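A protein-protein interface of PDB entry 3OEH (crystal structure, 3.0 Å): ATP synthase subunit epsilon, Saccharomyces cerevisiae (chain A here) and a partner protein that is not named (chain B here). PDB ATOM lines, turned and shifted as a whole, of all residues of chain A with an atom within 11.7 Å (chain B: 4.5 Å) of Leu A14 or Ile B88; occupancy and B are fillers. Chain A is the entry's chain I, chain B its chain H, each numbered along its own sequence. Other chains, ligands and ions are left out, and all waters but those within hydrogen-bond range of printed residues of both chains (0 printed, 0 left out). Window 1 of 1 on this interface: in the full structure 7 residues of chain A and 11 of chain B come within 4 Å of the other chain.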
ATOM      1  N   ILE A   8       6.543   5.778  -1.990  1.00  0.00           N
ATOM      2  CA  ILE A   8       5.381   5.737  -2.918  1.00  0.00           C
ATOM      3  C   ILE A   8       4.855   4.307  -3.068  1.00  0.00           C
ATOM      4  O   ILE A   8       5.602   3.397  -3.452  1.00  0.00           O
ATOM      5  CB  ILE A   8       5.739   6.316  -4.302  1.00  0.00           C
ATOM      6  N   SER A   9       3.571   4.126  -2.750  1.00  0.00           N
ATOM      7  CA  SER A   9       2.880   2.834  -2.805  1.00  0.00           C
ATOM      8  C   SER A   9       1.392   3.095  -2.621  1.00  0.00           C
ATOM      9  O   SER A   9       1.028   3.974  -1.852  1.00  0.00           O
ATOM     10  CB  SER A   9       3.367   1.914  -1.690  1.00  0.00           C
ATOM     11  OG  SER A   9       3.044   2.457  -0.420  1.00  0.00           O
ATOM     12  N   TYR A  10       0.541   2.319  -3.294  1.00  0.00           N
ATOM     13  CA  TYR A  10      -0.900   2.622  -3.384  1.00  0.00           C
ATOM     14  C   TYR A  10      -1.562   3.115  -2.081  1.00  0.00           C
ATOM     15  O   TYR A  10      -2.477   3.936  -2.123  1.00  0.00           O
ATOM     16  CB  TYR A  10      -1.692   1.450  -3.999  1.00  0.00           C
ATOM     17  CG  TYR A  10      -3.138   1.800  -4.333  1.00  0.00           C
ATOM     18  CD1 TYR A  10      -3.473   2.400  -5.552  1.00  0.00           C
ATOM     19  CD2 TYR A  10      -4.169   1.543  -3.424  1.00  0.00           C
ATOM     20  CE1 TYR A  10      -4.802   2.735  -5.857  1.00  0.00           C
ATOM     21  CE2 TYR A  10      -5.496   1.871  -3.720  1.00  0.00           C
ATOM     22  CZ  TYR A  10      -5.811   2.467  -4.936  1.00  0.00           C
ATOM     23  OH  TYR A  10      -7.126   2.795  -5.218  1.00  0.00           O
ATOM     24  N   ALA A  11      -1.103   2.617  -0.936  1.00  0.00           N
ATOM     25  CA  ALA A  11      -1.590   3.092   0.354  1.00  0.00           C
ATOM     26  C   ALA A  11      -1.036   4.488   0.651  1.00  0.00           C
ATOM     27  O   ALA A  11      -1.796   5.440   0.866  1.00  0.00           O
ATOM     28  CB  ALA A  11      -1.193   2.120   1.443  1.00  0.00           C
ATOM     29  N   ALA A  12       0.292   4.595   0.656  1.00  0.00           N
ATOM     30  CA  ALA A  12       1.002   5.858   0.856  1.00  0.00           C
ATOM     31  C   ALA A  12       0.640   6.895  -0.207  1.00  0.00           C
ATOM     32  O   ALA A  12       0.772   8.098   0.021  1.00  0.00           O
ATOM     33  CB  ALA A  12       2.510   5.613   0.864  1.00  0.00           C
ATOM     34  N   TYR A  13       0.185   6.410  -1.360  1.00  0.00           N
ATOM     35  CA  TYR A  13      -0.183   7.231  -2.512  1.00  0.00           C
ATOM     36  C   TYR A  13      -1.572   7.851  -2.345  1.00  0.00           C
ATOM     37  O   TYR A  13      -1.792   8.991  -2.740  1.00  0.00           O
ATOM     38  CB  TYR A  13      -0.079   6.383  -3.793  1.00  0.00           C
ATOM     39  CG  TYR A  13      -0.874   6.867  -4.986  1.00  0.00           C
ATOM     40  CD1 TYR A  13      -2.116   6.306  -5.291  1.00  0.00           C
ATOM     41  CD2 TYR A  13      -0.377   7.868  -5.825  1.00  0.00           C
ATOM     42  CE1 TYR A  13      -2.853   6.739  -6.385  1.00  0.00           C
ATOM     43  CE2 TYR A  13      -1.105   8.309  -6.926  1.00  0.00           C
ATOM     44  CZ  TYR A  13      -2.344   7.740  -7.199  1.00  0.00           C
ATOM     45  OH  TYR A  13      -3.072   8.167  -8.288  1.00  0.00           O
ATOM     46  N   LEU A  14      -2.501   7.102  -1.759  1.00  0.00           N
ATOM     47  CA  LEU A  14      -3.841   7.614  -1.469  1.00  0.00           C
ATOM     48  C   LEU A  14      -3.828   8.497  -0.235  1.00  0.00           C
ATOM     49  O   LEU A  14      -4.663   9.390  -0.096  1.00  0.00           O
ATOM     50  CB  LEU A  14      -4.839   6.472  -1.260  1.00  0.00           C
ATOM     51  CG  LEU A  14      -5.426   5.667  -2.424  1.00  0.00           C
ATOM     52  CD1 LEU A  14      -6.594   4.856  -1.903  1.00  0.00           C
ATOM     53  CD2 LEU A  14      -5.875   6.542  -3.589  1.00  0.00           C
ATOM     54  N   ASN A  15      -2.881   8.224   0.662  1.00  0.00           N
ATOM     55  CA  ASN A  15      -2.693   9.000   1.885  1.00  0.00           C
ATOM     56  C   ASN A  15      -2.299  10.454   1.615  1.00  0.00           C
ATOM     57  O   ASN A  15      -2.875  11.373   2.197  1.00  0.00           O
ATOM     58  CB  ASN A  15      -1.653   8.330   2.791  1.00  0.00           C
ATOM     59  CG  ASN A  15      -1.256   9.206   3.978  1.00  0.00           C
ATOM     60  OD1 ASN A  15      -0.134   9.716   4.039  1.00  0.00           O
ATOM     61  ND2 ASN A  15      -2.182   9.396   4.917  1.00  0.00           N
ATOM     62  N   VAL A  16      -1.314  10.654   0.739  1.00  0.00           N
ATOM     63  CA  VAL A  16      -0.886  12.002   0.362  1.00  0.00           C
ATOM     64  C   VAL A  16      -2.045  12.746  -0.321  1.00  0.00           C
ATOM     65  O   VAL A  16      -2.176  13.965  -0.187  1.00  0.00           O
ATOM     66  CB  VAL A  16       0.398  12.003  -0.525  1.00  0.00           C
ATOM     67  CG1 VAL A  16       1.036  13.399  -0.550  1.00  0.00           C
ATOM     68  CG2 VAL A  16       1.420  11.000  -0.011  1.00  0.00           C
ATOM     69  N   ALA A  17      -2.896  12.000  -1.025  1.00  0.00           N
ATOM     70  CA  ALA A  17      -4.144  12.542  -1.570  1.00  0.00           C
ATOM     71  C   ALA A  17      -5.188  12.802  -0.473  1.00  0.00           C
ATOM     72  O   ALA A  17      -6.115  13.592  -0.661  1.00  0.00           O
ATOM     73  CB  ALA A  17      -4.713  11.613  -2.638  1.00  0.00           C
ATOM     74  N   ALA A  18      -5.028  12.133   0.669  1.00  0.00           N
ATOM     75  CA  ALA A  18      -5.925  12.308   1.812  1.00  0.00           C
ATOM     76  C   ALA A  18      -5.433  13.431   2.741  1.00  0.00           C
ATOM     77  O   ALA A  18      -5.923  13.591   3.869  1.00  0.00           O
ATOM     78  CB  ALA A  18      -6.064  10.986   2.572  1.00  0.00           C
ATOM     79  N   GLN A  19      -4.466  14.203   2.249  1.00  0.00           N
ATOM     80  CA  GLN A  19      -3.865  15.296   3.008  1.00  0.00           C
ATOM     81  C   GLN A  19      -3.888  16.602   2.238  1.00  0.00           C
ATOM     82  O   GLN A  19      -3.467  17.640   2.750  1.00  0.00           O
ATOM     83  CB  GLN A  19      -2.433  14.951   3.418  1.00  0.00           C
ATOM     84  CG  GLN A  19      -2.343  14.199   4.733  1.00  0.00           C
ATOM     85  CD  GLN A  19      -2.518  15.105   5.937  1.00  0.00           C
ATOM     86  OE1 GLN A  19      -3.517  15.822   6.063  1.00  0.00           O
ATOM     87  NE2 GLN A  19      -1.543  15.073   6.833  1.00  0.00           N
ATOM     88  N   ALA A  20      -4.356  16.537   0.996  1.00  0.00           N
ATOM     89  CA  ALA A  20      -4.710  17.733   0.246  1.00  0.00           C
ATOM     90  C   ALA A  20      -6.166  18.043   0.584  1.00  0.00           C
ATOM     91  O   ALA A  20      -6.515  19.185   0.902  1.00  0.00           O
ATOM     92  CB  ALA A  20      -4.534  17.502  -1.244  1.00  0.00           C
ATOM     93  N   ILE A  21      -6.993  16.997   0.537  1.00  0.00           N
ATOM     94  CA  ILE A  21      -8.401  17.049   0.933  1.00  0.00           C
ATOM     95  C   ILE A  21      -8.544  17.212   2.444  1.00  0.00           C
ATOM     96  O   ILE A  21      -9.654  17.220   2.979  1.00  0.00           O
ATOM     97  CB  ILE A  21      -9.154  15.769   0.486  1.00  0.00           C
ATOM     98  N   ARG A  22      -7.406  17.329   3.120  1.00  0.00           N
ATOM     99  CA  ARG A  22      -7.354  17.531   4.561  1.00  0.00           C
ATOM    100  C   ARG A  22      -6.514  18.770   4.915  1.00  0.00           C
ATOM    101  O   ARG A  22      -6.592  19.287   6.037  1.00  0.00           O
ATOM    102  CB  ARG A  22      -6.804  16.276   5.248  1.00  0.00           C
ATOM    103  N   SER A  23      -5.721  19.236   3.947  1.00  0.00           N
ATOM    104  CA  SER A  23      -4.876  20.422   4.105  1.00  0.00           C
ATOM    105  C   SER A  23      -4.627  21.108   2.759  1.00  0.00           C
ATOM    106  O   SER A  23      -4.590  22.338   2.669  1.00  0.00           O
ATOM    107  CB  SER A  23      -3.544  20.051   4.771  1.00  0.00           C
ATOM    108  N   SER A  33     -10.499  16.172  14.899  1.00  0.00           N
ATOM    109  CA  SER A  33      -9.944  14.884  14.465  1.00  0.00           C
ATOM    110  C   SER A  33      -9.492  14.824  12.987  1.00  0.00           C
ATOM    111  O   SER A  33      -9.010  13.786  12.530  1.00  0.00           O
ATOM    112  CB  SER A  33     -10.918  13.741  14.785  1.00  0.00           C
ATOM    113  OG  SER A  33     -12.013  13.718  13.886  1.00  0.00           O
ATOM    114  N   VAL A  34      -9.659  15.923  12.249  1.00  0.00           N
ATOM    115  CA  VAL A  34      -9.131  16.039  10.881  1.00  0.00           C
ATOM    116  C   VAL A  34      -7.630  16.349  10.931  1.00  0.00           C
ATOM    117  O   VAL A  34      -6.825  15.675  10.282  1.00  0.00           O
ATOM    118  CB  VAL A  34      -9.893  17.112  10.060  1.00  0.00           C
ATOM    119  CG1 VAL A  34      -9.313  17.248   8.656  1.00  0.00           C
ATOM    120  CG2 VAL A  34     -11.374  16.774   9.987  1.00  0.00           C
ATOM    121  N   ASN A  36      -5.906  15.592  13.287  1.00  0.00           N
ATOM    122  CA  ASN A  36      -5.382  14.523  14.140  1.00  0.00           C
ATOM    123  C   ASN A  36      -5.342  13.202  13.373  1.00  0.00           C
ATOM    124  O   ASN A  36      -4.663  12.248  13.776  1.00  0.00           O
ATOM    125  CB  ASN A  36      -6.181  14.406  15.445  1.00  0.00           C
ATOM    126  CG  ASN A  36      -5.607  15.281  16.578  1.00  0.00           C
ATOM    127  OD1 ASN A  36      -5.406  16.493  16.424  1.00  0.00           O
ATOM    128  ND2 ASN A  36      -5.357  14.659  17.727  1.00  0.00           N
ATOM    129  N   ARG A  37      -6.086  13.169  12.267  1.00  0.00           N
ATOM    130  CA  ARG A  37      -5.919  12.175  11.208  1.00  0.00           C
ATOM    131  C   ARG A  37      -4.600  12.453  10.491  1.00  0.00           C
ATOM    132  O   ARG A  37      -4.008  11.562   9.869  1.00  0.00           O
ATOM    133  CB  ARG A  37      -7.077  12.271  10.205  1.00  0.00           C
ATOM    134  CG  ARG A  37      -6.698  11.995   8.733  1.00  0.00           C
ATOM    135  CD  ARG A  37      -7.810  12.331   7.748  1.00  0.00           C
ATOM    136  NE  ARG A  37      -9.108  11.858   8.223  1.00  0.00           N
ATOM    137  CZ  ARG A  37     -10.142  12.647   8.507  1.00  0.00           C
ATOM    138  NH1 ARG A  37     -10.059  13.961   8.337  1.00  0.00           N
ATOM    139  NH2 ARG A  37     -11.273  12.116   8.949  1.00  0.00           N
ATOM    140  N   SER A  38      -4.148  13.699  10.593  1.00  0.00           N
ATOM    141  CA  SER A  38      -3.002  14.178   9.835  1.00  0.00           C
ATOM    142  C   SER A  38      -1.665  14.019  10.571  1.00  0.00           C
ATOM    143  O   SER A  38      -0.608  13.950   9.937  1.00  0.00           O
ATOM    144  CB  SER A  38      -3.240  15.633   9.421  1.00  0.00           C
ATOM    145  OG  SER A  38      -4.370  15.728   8.561  1.00  0.00           O
ATOM    146  N   LEU B  16     -16.140   4.545   4.627  1.00  0.00           N
ATOM    147  CA  LEU B  16     -14.844   5.162   4.935  1.00  0.00           C
ATOM    148  C   LEU B  16     -14.329   4.624   6.280  1.00  0.00           C
ATOM    149  O   LEU B  16     -15.132   4.151   7.095  1.00  0.00           O
ATOM    150  CB  LEU B  16     -14.973   6.688   5.002  1.00  0.00           C
ATOM    151  CG  LEU B  16     -15.887   7.410   4.011  1.00  0.00           C
ATOM    152  CD1 LEU B  16     -16.348   8.739   4.593  1.00  0.00           C
ATOM    153  CD2 LEU B  16     -15.200   7.611   2.670  1.00  0.00           C
ATOM    154  N   PRO B  17     -12.997   4.699   6.525  1.00  0.00           N
ATOM    155  CA  PRO B  17     -12.448   4.197   7.789  1.00  0.00           C
ATOM    156  C   PRO B  17     -12.849   5.047   8.993  1.00  0.00           C
ATOM    157  O   PRO B  17     -13.029   4.499  10.080  1.00  0.00           O
ATOM    158  CB  PRO B  17     -10.936   4.262   7.570  1.00  0.00           C
ATOM    159  CG  PRO B  17     -10.746   5.346   6.579  1.00  0.00           C
ATOM    160  CD  PRO B  17     -11.944   5.294   5.677  1.00  0.00           C
ATOM    161  N   HIS B  18     -12.985   6.363   8.804  1.00  0.00           N
ATOM    162  CA  HIS B  18     -13.445   7.241   9.882  1.00  0.00           C
ATOM    163  C   HIS B  18     -14.960   7.402   9.951  1.00  0.00           C
ATOM    164  O   HIS B  18     -15.545   7.221  11.014  1.00  0.00           O
ATOM    165  CB  HIS B  18     -12.722   8.605   9.899  1.00  0.00           C
ATOM    166  CG  HIS B  18     -12.727   9.341   8.590  1.00  0.00           C
ATOM    167  ND1 HIS B  18     -13.749  10.186   8.213  1.00  0.00           N
ATOM    168  CD2 HIS B  18     -11.804   9.404   7.600  1.00  0.00           C
ATOM    169  CE1 HIS B  18     -13.470  10.716   7.036  1.00  0.00           C
ATOM    170  NE2 HIS B  18     -12.292  10.262   6.644  1.00  0.00           N
ATOM    171  N   SER B  71     -10.893  10.698  -1.709  1.00  0.00           N
ATOM    172  CA  SER B  71      -9.452  10.497  -1.686  1.00  0.00           C
ATOM    173  C   SER B  71      -9.059   9.430  -2.698  1.00  0.00           C
ATOM    174  O   SER B  71      -8.093   9.587  -3.452  1.00  0.00           O
ATOM    175  CB  SER B  71      -9.012  10.062  -0.286  1.00  0.00           C
ATOM    176  OG  SER B  71      -9.768   8.944   0.167  1.00  0.00           O
ATOM    177  N   GLY B  72      -9.821   8.343  -2.700  1.00  0.00           N
ATOM    178  CA  GLY B  72      -9.574   7.223  -3.584  1.00  0.00           C
ATOM    179  C   GLY B  72      -9.966   5.927  -2.915  1.00  0.00           C
ATOM    180  O   GLY B  72     -10.551   5.924  -1.832  1.00  0.00           O
ATOM    181  N   GLY B  73      -9.639   4.820  -3.571  1.00  0.00           N
ATOM    182  CA  GLY B  73      -9.937   3.511  -3.030  1.00  0.00           C
ATOM    183  C   GLY B  73     -10.395   2.575  -4.113  1.00  0.00           C
ATOM    184  O   GLY B  73      -9.837   2.575  -5.206  1.00  0.00           O
ATOM    185  N   ALA B  87     -13.368   4.422   0.478  1.00  0.00           N
ATOM    186  CA  ALA B  87     -12.459   5.550   0.341  1.00  0.00           C
ATOM    187  C   ALA B  87     -11.946   5.905   1.722  1.00  0.00           C
ATOM    188  O   ALA B  87     -12.559   5.537   2.724  1.00  0.00           O
ATOM    189  CB  ALA B  87     -13.167   6.733  -0.282  1.00  0.00           C
ATOM    190  N   ILE B  88     -10.811   6.596   1.771  1.00  0.00           N
ATOM    191  CA  ILE B  88     -10.264   7.080   3.034  1.00  0.00           C
ATOM    192  C   ILE B  88     -11.033   8.326   3.458  1.00  0.00           C
ATOM    193  O   ILE B  88     -11.435   8.456   4.617  1.00  0.00           O
ATOM    194  CB  ILE B  88      -8.768   7.438   2.916  1.00  0.00           C
ATOM    195  CG1 ILE B  88      -8.002   6.340   2.171  1.00  0.00           C
ATOM    196  CG2 ILE B  88      -8.166   7.717   4.298  1.00  0.00           C
ATOM    197  CD1 ILE B  88      -6.930   6.889   1.263  1.00  0.00           C
ATOM    198  N   GLU B  89     -11.243   9.222   2.495  1.00  0.00           N
ATOM    199  CA  GLU B  89     -11.826  10.536   2.736  1.00  0.00           C
ATOM    200  C   GLU B  89     -13.049  10.773   1.858  1.00  0.00           C
ATOM    201  O   GLU B  89     -13.068  10.372   0.692  1.00  0.00           O
ATOM    202  CB  GLU B  89     -10.793  11.636   2.448  1.00  0.00           C
ATOM    203  CG  GLU B  89      -9.540  11.618   3.317  1.00  0.00           C
ATOM    204  CD  GLU B  89      -9.658  12.519   4.525  1.00  0.00           C
ATOM    205  OE1 GLU B  89     -10.618  12.336   5.307  1.00  0.00           O
ATOM    206  OE2 GLU B  89      -8.792  13.412   4.690  1.00  0.00           O
ATOM    207  N   ALA B  90     -14.055  11.443   2.421  1.00  0.00           N
ATOM    208  CA  ALA B  90     -15.212  11.926   1.663  1.00  0.00           C
ATOM    209  C   ALA B  90     -15.304  13.453   1.705  1.00  0.00           C
ATOM    210  O   ALA B  90     -14.287  14.153   1.693  1.00  0.00           O
ATOM    211  CB  ALA B  90     -16.488  11.314   2.189  1.00  0.00           C
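NE2 of His B18 lies close to NH2 of Arg A37. The side-chain hydroxyl of Tyr A10 lies within hydrogen-bond range of the backbone carbonyl oxygen of Gly B73. The side-chain carboxylate of Glu B89 lies within salt-bridge range of the guanidinium group of Arg A37 (3.3 Å). O of Ala A18 lies close to OE2 of Glu B89.
The backbone carbonyl oxygen of Ile B88 lies within hydrogen-bond range of a ring nitrogen (NE2) of His B18. A ring nitrogen (NE2) of His B18 sits at hydrogen-bond distance from the side-chain carboxylate (OE1) of Glu B89 (3.0 Å). N of Ile B88 lies within hydrogen-bond range of OG of Ser B71 (3.0 Å). The side-chain hydroxyl (OG) of Ser B71 lies within hydrogen-bond range of the backbone NH (N) of Glu B89 (2.8 Å).
Among the printed residues, pairs that only touch across the chains: Leu A14 with Ile B88 (3.3 Å), Leu A14 with Gly B73 (3.5 Å), Arg A22 with Glu B89 (3.5 Å), Leu A14 with Gly B72 (3.7 Å) and Leu A14 with Ser B71 (3.8 Å).
Leu A14 touches just these residues of chain B: Ser B71 (3.8 Å), Gly B72 (3.7 Å), Gly B73 (3.5 Å) and Ile B88 (3.3 Å). No residue of chain A comes within 4 Å of Leu B16. Of the printed residues of chain A, Ser B71 touches Leu A14. Of the printed residues of chain A, Gly B72 touches Leu A14 (3.7 Å). Of chain A, only Tyr A10 and Leu A14 come within 4 Å of Gly B73. No residue of chain A comes within 4 Å of Ala B87. No residue of chain A comes within 4 Å of Ala B90. Printed residues of chain B within 4 Å of Arg A37: His B18 (3.1 Å) and Glu B89 (3.3 Å). Of the printed residues of chain B, Tyr A10 touches Gly B73. Ile A21 touches none of the printed residues of chain B. Ile A8 touches none of the printed residues of chain B.
Hydrophobic or aromatic side chains of chain B that line the printed part of chain A: His B18 and Ile B88. Among the printed residues, 9 pairs touch across the chains. Among the printed residues, Asp or Glu carboxylates within 4 Å of a Lys or Arg side-chain nitrogen of the other chain: Arg A37 with Glu B89.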
